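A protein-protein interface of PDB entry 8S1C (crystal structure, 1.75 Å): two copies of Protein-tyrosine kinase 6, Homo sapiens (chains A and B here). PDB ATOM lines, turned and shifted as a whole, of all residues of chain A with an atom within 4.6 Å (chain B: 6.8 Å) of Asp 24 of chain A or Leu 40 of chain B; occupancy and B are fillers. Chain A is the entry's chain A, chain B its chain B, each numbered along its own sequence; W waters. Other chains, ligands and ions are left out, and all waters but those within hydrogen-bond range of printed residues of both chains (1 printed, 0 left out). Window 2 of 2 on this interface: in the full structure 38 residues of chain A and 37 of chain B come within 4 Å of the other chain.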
ATOM      1  N   TYR A   4      -0.873   2.510  -2.097  1.00  0.00           N
ATOM      2  CA  TYR A   4      -2.093   3.282  -2.251  1.00  0.00           C
ATOM      3  C   TYR A   4      -2.073   4.413  -1.242  1.00  0.00           C
ATOM      4  O   TYR A   4      -1.356   4.347  -0.249  1.00  0.00           O
ATOM      5  CB  TYR A   4      -3.326   2.408  -2.013  1.00  0.00           C
ATOM      6  CG  TYR A   4      -3.414   1.258  -2.976  1.00  0.00           C
ATOM      7  CD1 TYR A   4      -2.698   0.078  -2.761  1.00  0.00           C
ATOM      8  CD2 TYR A   4      -4.208   1.350  -4.108  1.00  0.00           C
ATOM      9  CE1 TYR A   4      -2.783  -0.973  -3.664  1.00  0.00           C
ATOM     10  CE2 TYR A   4      -4.305   0.303  -4.990  1.00  0.00           C
ATOM     11  CZ  TYR A   4      -3.576  -0.838  -4.784  1.00  0.00           C
ATOM     12  OH  TYR A   4      -3.672  -1.870  -5.698  1.00  0.00           O
ATOM     13  N   VAL A   5      -2.883   5.448  -1.491  1.00  0.00           N
ATOM     14  CA  VAL A   5      -3.019   6.587  -0.587  1.00  0.00           C
ATOM     15  C   VAL A   5      -4.482   6.719  -0.200  1.00  0.00           C
ATOM     16  O   VAL A   5      -5.384   6.501  -1.025  1.00  0.00           O
ATOM     17  CB  VAL A   5      -2.495   7.885  -1.236  1.00  0.00           C
ATOM     18  CG1 VAL A   5      -3.377   8.293  -2.423  1.00  0.00           C
ATOM     19  CG2 VAL A   5      -2.423   9.001  -0.230  1.00  0.00           C
ATOM     20  N   GLY A   6      -4.717   7.053   1.067  1.00  0.00           N
ATOM     21  CA  GLY A   6      -6.072   7.229   1.542  1.00  0.00           C
ATOM     22  C   GLY A   6      -6.598   8.581   1.121  1.00  0.00           C
ATOM     23  O   GLY A   6      -5.911   9.602   1.250  1.00  0.00           O
ATOM     24  N   LEU A  18      -9.301  -0.941  10.092  1.00  0.00           N
ATOM     25  CA  LEU A  18      -8.122  -0.127  10.383  1.00  0.00           C
ATOM     26  C   LEU A  18      -8.468   1.339  10.177  1.00  0.00           C
ATOM     27  O   LEU A  18      -8.788   1.739   9.058  1.00  0.00           O
ATOM     28  CB  LEU A  18      -6.962  -0.538   9.482  1.00  0.00           C
ATOM     29  CG  LEU A  18      -5.710   0.341   9.416  1.00  0.00           C
ATOM     30  CD1 LEU A  18      -5.077   0.469  10.786  1.00  0.00           C
ATOM     31  CD2 LEU A  18      -4.723  -0.205   8.419  1.00  0.00           C
ATOM     32  N   PHE A  20      -7.640   5.329   9.732  1.00  0.00           N
ATOM     33  CA  PHE A  20      -6.547   6.054   9.099  1.00  0.00           C
ATOM     34  C   PHE A  20      -6.971   7.474   8.743  1.00  0.00           C
ATOM     35  O   PHE A  20      -8.134   7.863   8.892  1.00  0.00           O
ATOM     36  CB  PHE A  20      -6.029   5.314   7.842  1.00  0.00           C
ATOM     37  CG  PHE A  20      -7.056   5.124   6.755  1.00  0.00           C
ATOM     38  CD1 PHE A  20      -7.271   6.097   5.785  1.00  0.00           C
ATOM     39  CD2 PHE A  20      -7.783   3.948   6.689  1.00  0.00           C
ATOM     40  CE1 PHE A  20      -8.191   5.878   4.750  1.00  0.00           C
ATOM     41  CE2 PHE A  20      -8.721   3.738   5.675  1.00  0.00           C
ATOM     42  CZ  PHE A  20      -8.912   4.691   4.704  1.00  0.00           C
ATOM     43  N   ARG A  21      -5.996   8.255   8.319  1.00  0.00           N
ATOM     44  CA  ARG A  21      -6.206   9.645   7.958  1.00  0.00           C
ATOM     45  C   ARG A  21      -5.979   9.834   6.468  1.00  0.00           C
ATOM     46  O   ARG A  21      -5.203   9.103   5.834  1.00  0.00           O
ATOM     47  CB  ARG A  21      -5.258  10.553   8.744  1.00  0.00           C
ATOM     48  CG  ARG A  21      -5.370  10.382  10.258  1.00  0.00           C
ATOM     49  CD  ARG A  21      -4.094  10.904  10.908  1.00  0.00           C
ATOM     50  NE  ARG A  21      -4.184  11.099  12.352  1.00  0.00           N
ATOM     51  CZ  ARG A  21      -4.725  12.161  12.938  1.00  0.00           C
ATOM     52  NH1 ARG A  21      -5.386  13.078  12.244  1.00  0.00           N
ATOM     53  NH2 ARG A  21      -4.596  12.313  14.252  1.00  0.00           N
ATOM     54  N   ALA A  22      -6.648  10.835   5.914  1.00  0.00           N
ATOM     55  CA  ALA A  22      -6.365  11.238   4.544  1.00  0.00           C
ATOM     56  C   ALA A  22      -4.868  11.442   4.336  1.00  0.00           C
ATOM     57  O   ALA A  22      -4.201  12.117   5.126  1.00  0.00           O
ATOM     58  CB  ALA A  22      -7.115  12.526   4.204  1.00  0.00           C
ATOM     59  N   GLY A  23      -4.347  10.860   3.261  1.00  0.00           N
ATOM     60  CA  GLY A  23      -2.946  10.968   2.925  1.00  0.00           C
ATOM     61  C   GLY A  23      -2.075   9.843   3.425  1.00  0.00           C
ATOM     62  O   GLY A  23      -0.904   9.772   3.037  1.00  0.00           O
ATOM     63  N   ASP A  24      -2.595   8.976   4.294  1.00  0.00           N
ATOM     64  CA  ASP A  24      -1.833   7.815   4.748  1.00  0.00           C
ATOM     65  C   ASP A  24      -1.558   6.889   3.578  1.00  0.00           C
ATOM     66  O   ASP A  24      -2.334   6.814   2.625  1.00  0.00           O
ATOM     67  CB  ASP A  24      -2.592   7.073   5.847  1.00  0.00           C
ATOM     68  CG  ASP A  24      -2.495   7.763   7.173  1.00  0.00           C
ATOM     69  OD1 ASP A  24      -1.698   8.732   7.270  1.00  0.00           O
ATOM     70  OD2 ASP A  24      -3.235   7.363   8.094  1.00  0.00           O
ATOM     71  N   VAL A  25      -0.416   6.200   3.638  1.00  0.00           N
ATOM     72  CA  VAL A  25       0.037   5.342   2.556  1.00  0.00           C
ATOM     73  C   VAL A  25      -0.087   3.903   3.018  1.00  0.00           C
ATOM     74  O   VAL A  25       0.234   3.581   4.164  1.00  0.00           O
ATOM     75  CB  VAL A  25       1.487   5.639   2.131  1.00  0.00           C
ATOM     76  CG1 VAL A  25       1.930   4.653   1.020  1.00  0.00           C
ATOM     77  CG2 VAL A  25       1.592   7.067   1.663  1.00  0.00           C
ATOM     78  N   PHE A  26      -0.530   3.038   2.121  1.00  0.00           N
ATOM     79  CA  PHE A  26      -0.767   1.651   2.453  1.00  0.00           C
ATOM     80  C   PHE A  26      -0.028   0.751   1.485  1.00  0.00           C
ATOM     81  O   PHE A  26       0.193   1.110   0.334  1.00  0.00           O
ATOM     82  CB  PHE A  26      -2.256   1.274   2.357  1.00  0.00           C
ATOM     83  CG  PHE A  26      -3.123   2.067   3.251  1.00  0.00           C
ATOM     84  CD1 PHE A  26      -3.610   3.295   2.853  1.00  0.00           C
ATOM     85  CD2 PHE A  26      -3.455   1.583   4.506  1.00  0.00           C
ATOM     86  CE1 PHE A  26      -4.400   4.024   3.686  1.00  0.00           C
ATOM     87  CE2 PHE A  26      -4.257   2.318   5.335  1.00  0.00           C
ATOM     88  CZ  PHE A  26      -4.720   3.534   4.923  1.00  0.00           C
ATOM     89  N   ALA B  38      -5.217  -4.295   4.431  1.00  0.00           N
ATOM     90  CA  ALA B  38      -4.133  -3.393   4.070  1.00  0.00           C
ATOM     91  C   ALA B  38      -3.154  -3.265   5.229  1.00  0.00           C
ATOM     92  O   ALA B  38      -3.500  -3.539   6.377  1.00  0.00           O
ATOM     93  CB  ALA B  38      -4.669  -2.000   3.719  1.00  0.00           C
ATOM     94  N   THR B  39      -1.929  -2.851   4.905  1.00  0.00           N
ATOM     95  CA  THR B  39      -0.923  -2.476   5.897  1.00  0.00           C
ATOM     96  C   THR B  39      -0.659  -0.976   5.809  1.00  0.00           C
ATOM     97  O   THR B  39      -0.299  -0.468   4.746  1.00  0.00           O
ATOM     98  CB  THR B  39       0.367  -3.243   5.690  1.00  0.00           C
ATOM     99  OG1 THR B  39       0.081  -4.657   5.686  1.00  0.00           O
ATOM    100  CG2 THR B  39       1.367  -2.920   6.783  1.00  0.00           C
ATOM    101  N   LEU B  40      -0.850  -0.281   6.915  1.00  0.00           N
ATOM    102  CA  LEU B  40      -0.528   1.141   7.009  1.00  0.00           C
ATOM    103  C   LEU B  40       0.976   1.308   7.148  1.00  0.00           C
ATOM    104  O   LEU B  40       1.615   0.612   7.940  1.00  0.00           O
ATOM    105  CB  LEU B  40      -1.245   1.765   8.197  1.00  0.00           C
ATOM    106  CG  LEU B  40      -0.938   3.235   8.518  1.00  0.00           C
ATOM    107  CD1 LEU B  40      -1.399   4.144   7.406  1.00  0.00           C
ATOM    108  CD2 LEU B  40      -1.609   3.590   9.824  1.00  0.00           C
ATOM    109  N   LEU B  41       1.543   2.223   6.374  1.00  0.00           N
ATOM    110  CA  LEU B  41       2.965   2.511   6.431  1.00  0.00           C
ATOM    111  C   LEU B  41       3.212   3.794   7.205  1.00  0.00           C
ATOM    112  O   LEU B  41       2.379   4.718   7.231  1.00  0.00           O
ATOM    113  CB  LEU B  41       3.549   2.643   5.032  1.00  0.00           C
ATOM    114  CG  LEU B  41       3.193   1.478   4.139  1.00  0.00           C
ATOM    115  CD1 LEU B  41       3.899   1.663   2.808  1.00  0.00           C
ATOM    116  CD2 LEU B  41       3.593   0.175   4.780  1.00  0.00           C
ATOM    117  N   ASP B  42       4.349   3.843   7.879  1.00  0.00           N
ATOM    118  CA  ASP B  42       4.709   5.093   8.527  1.00  0.00           C
ATOM    119  C   ASP B  42       5.410   5.987   7.510  1.00  0.00           C
ATOM    120  O   ASP B  42       5.560   5.643   6.342  1.00  0.00           O
ATOM    121  CB  ASP B  42       5.545   4.847   9.784  1.00  0.00           C
ATOM    122  CG  ASP B  42       6.900   4.253   9.498  1.00  0.00           C
ATOM    123  OD1 ASP B  42       7.320   4.209   8.325  1.00  0.00           O
ATOM    124  OD2 ASP B  42       7.562   3.820  10.479  1.00  0.00           O
ATOM    125  N   GLY B  45       7.939   4.433   5.389  1.00  0.00           N
ATOM    126  CA  GLY B  45       7.609   3.306   4.542  1.00  0.00           C
ATOM    127  C   GLY B  45       7.528   1.972   5.245  1.00  0.00           C
ATOM    128  O   GLY B  45       7.452   0.938   4.570  1.00  0.00           O
ATOM    129  N   GLY B  46       7.525   1.948   6.579  1.00  0.00           N
ATOM    130  CA  GLY B  46       7.474   0.708   7.328  1.00  0.00           C
ATOM    131  C   GLY B  46       6.067   0.364   7.819  1.00  0.00           C
ATOM    132  O   GLY B  46       5.285   1.237   8.136  1.00  0.00           O
ATOM    133  N   ALA B  47       5.772  -0.926   7.870  1.00  0.00           N
ATOM    134  CA  ALA B  47       4.464  -1.360   8.359  1.00  0.00           C
ATOM    135  C   ALA B  47       4.265  -0.977   9.813  1.00  0.00           C
ATOM    136  O   ALA B  47       5.128  -1.282  10.637  1.00  0.00           O
ATOM    137  CB  ALA B  47       4.364  -2.876   8.225  1.00  0.00           C
ATOM    138  N   VAL B  48       3.103  -0.357  10.140  1.00  0.00           N
ATOM    139  CA  VAL B  48       2.780   0.020  11.521  1.00  0.00           C
ATOM    140  C   VAL B  48       1.383  -0.402  11.953  1.00  0.00           C
ATOM    141  O   VAL B  48       1.062  -0.399  13.147  1.00  0.00           O
ATOM    142  CB  VAL B  48       2.929   1.552  11.762  1.00  0.00           C
ATOM    143  CG1 VAL B  48       4.371   1.925  11.734  1.00  0.00           C
ATOM    144  CG2 VAL B  48       2.148   2.355  10.738  1.00  0.00           C
ATOM    145  N   ALA B  49       0.542  -0.841  11.006  1.00  0.00           N
ATOM    146  CA  ALA B  49      -0.779  -1.307  11.393  1.00  0.00           C
ATOM    147  C   ALA B  49      -1.342  -2.118  10.232  1.00  0.00           C
ATOM    148  O   ALA B  49      -0.870  -2.001   9.097  1.00  0.00           O
ATOM    149  CB  ALA B  49      -1.697  -0.150  11.789  1.00  0.00           C
ATOM    150  N   GLN B  50      -2.308  -2.974  10.553  1.00  0.00           N
ATOM    151  CA  GLN B  50      -2.979  -3.809   9.556  1.00  0.00           C
ATOM    152  C   GLN B  50      -4.463  -3.843   9.866  1.00  0.00           C
ATOM    153  O   GLN B  50      -4.873  -3.754  11.029  1.00  0.00           O
ATOM    154  CB  GLN B  50      -2.469  -5.267   9.531  1.00  0.00           C
ATOM    155  CG  GLN B  50      -1.049  -5.443   9.115  1.00  0.00           C
ATOM    156  CD  GLN B  50      -0.665  -6.898   9.027  1.00  0.00           C
ATOM    157  OE1 GLN B  50      -1.474  -7.740   8.623  1.00  0.00           O
ATOM    158  NE2 GLN B  50       0.577  -7.216   9.402  1.00  0.00           N
ATOM    159  N   GLY B  51      -5.265  -4.038   8.844  1.00  0.00           N
ATOM    160  CA  GLY B  51      -6.690  -4.158   9.043  1.00  0.00           C
ATOM    161  C   GLY B  51      -7.449  -3.946   7.752  1.00  0.00           C
ATOM    162  O   GLY B  51      -6.889  -3.615   6.726  1.00  0.00           O
ATOM    163  N   LEU B  58      -9.143   4.358  -1.156  1.00  0.00           N
ATOM    164  CA  LEU B  58      -7.744   4.314  -1.541  1.00  0.00           C
ATOM    165  C   LEU B  58      -7.592   4.656  -3.013  1.00  0.00           C
ATOM    166  O   LEU B  58      -8.419   4.272  -3.840  1.00  0.00           O
ATOM    167  CB  LEU B  58      -7.143   2.922  -1.279  1.00  0.00           C
ATOM    168  CG  LEU B  58      -6.523   2.696   0.110  1.00  0.00           C
ATOM    169  CD1 LEU B  58      -7.437   3.100   1.223  1.00  0.00           C
ATOM    170  CD2 LEU B  58      -6.103   1.217   0.260  1.00  0.00           C
HETATM  171  O   HOH W   1       1.621   6.901   5.562  1.00  0.00           O
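Water W1 lies within hydrogen-bond range of O of Leu 41 of chain B (2.9 Å) and N of Val 25 of chain A (2.9 Å).
Of the printed residues of chain B, Tyr 4 of chain A touches Leu 58. Gly 6 of chain A touches none of the printed residues of chain B. Of chain B, only Leu 40 comes within 4 Å of Asp 24 of chain A. Of the printed residues of chain B, Phe 26 of chain A touches Ala 38 (3.9 Å), Thr 39 (3.2 Å) and Leu 40 (3.9 Å). Printed residues of chain A within 4 Å of Leu 40 of chain B: Asp 24, Val 25 and Phe 26. The nearest printed residue of chain A that does not touch Leu 40 of chain B is Leu 18 of chain A (4.003 Å). The nearest printed residue of chain A that does not touch Leu 41 of chain B is Phe 26 of chain A (4.2 Å).
Among the printed residues, merely in contact across the chains: Tyr 4 of chain A with Leu 58 of chain B (3.8 Å), Val 5 of chain A with Leu 58 of chain B (3.3 Å), Leu 18 of chain A with Ala 49 of chain B (3.6 Å), Leu 18 of chain A with Gln 50 of chain B (3.9 Å), Leu 18 of chain A with Gly 51 of chain B (3.7 Å), Asp 24 of chain A with Leu 40 of chain B (3.5 Å), Val 25 of chain A with Leu 40 of chain B (3.7 Å), Phe 26 of chain A with Ala 38 of chain B (3.9 Å), Phe 26 of chain A with Thr 39 of chain B (3.2 Å) and Phe 26 of chain A with Leu 40 of chain B (3.9 Å).
OD2 of Asp 24 of chain A sits at hydrogen-bond distance from N of Arg 21 of chain A. N of Leu 40 of chain B lies within hydrogen-bond range of O of Ala 49 of chain B. The backbone NH (N) of Gly 6 of chain A sits at hydrogen-bond distance from the backbone carbonyl oxygen (O) of Asp 24 of chain A, 2.9 Å away. The backbone carbonyl oxygen (O) of Gly 51 of chain B is in hydrogen-bond range of the backbone NH (N) of Ala 38 of chain B (2.9 Å). The backbone carbonyl oxygen (O) of Tyr 4 of chain A is in hydrogen-bond range of the backbone NH (N) of Phe 26 of chain A, at 2.8 Å. The backbone carbonyl oxygen of Leu 40 of chain B lies within hydrogen-bond range of the backbone NH of Val 48 of chain B (2.8 Å).
Hydrophobic or aromatic side chains of chain A that line the printed part of chain B: Tyr 4, Leu 18 and Phe 26. Of the 13 printed residues of chain B, 8 touch a printed residue of chain A. Among the printed residues, no Asp or Glu carboxylate lies within 4 Å of a Lys or Arg side-chain nitrogen of the other chain.
O of Val 25 of chain A is in hydrogen-bond range of N of Leu 41 of chain B (2.9 Å).
No position is printed for both chains.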
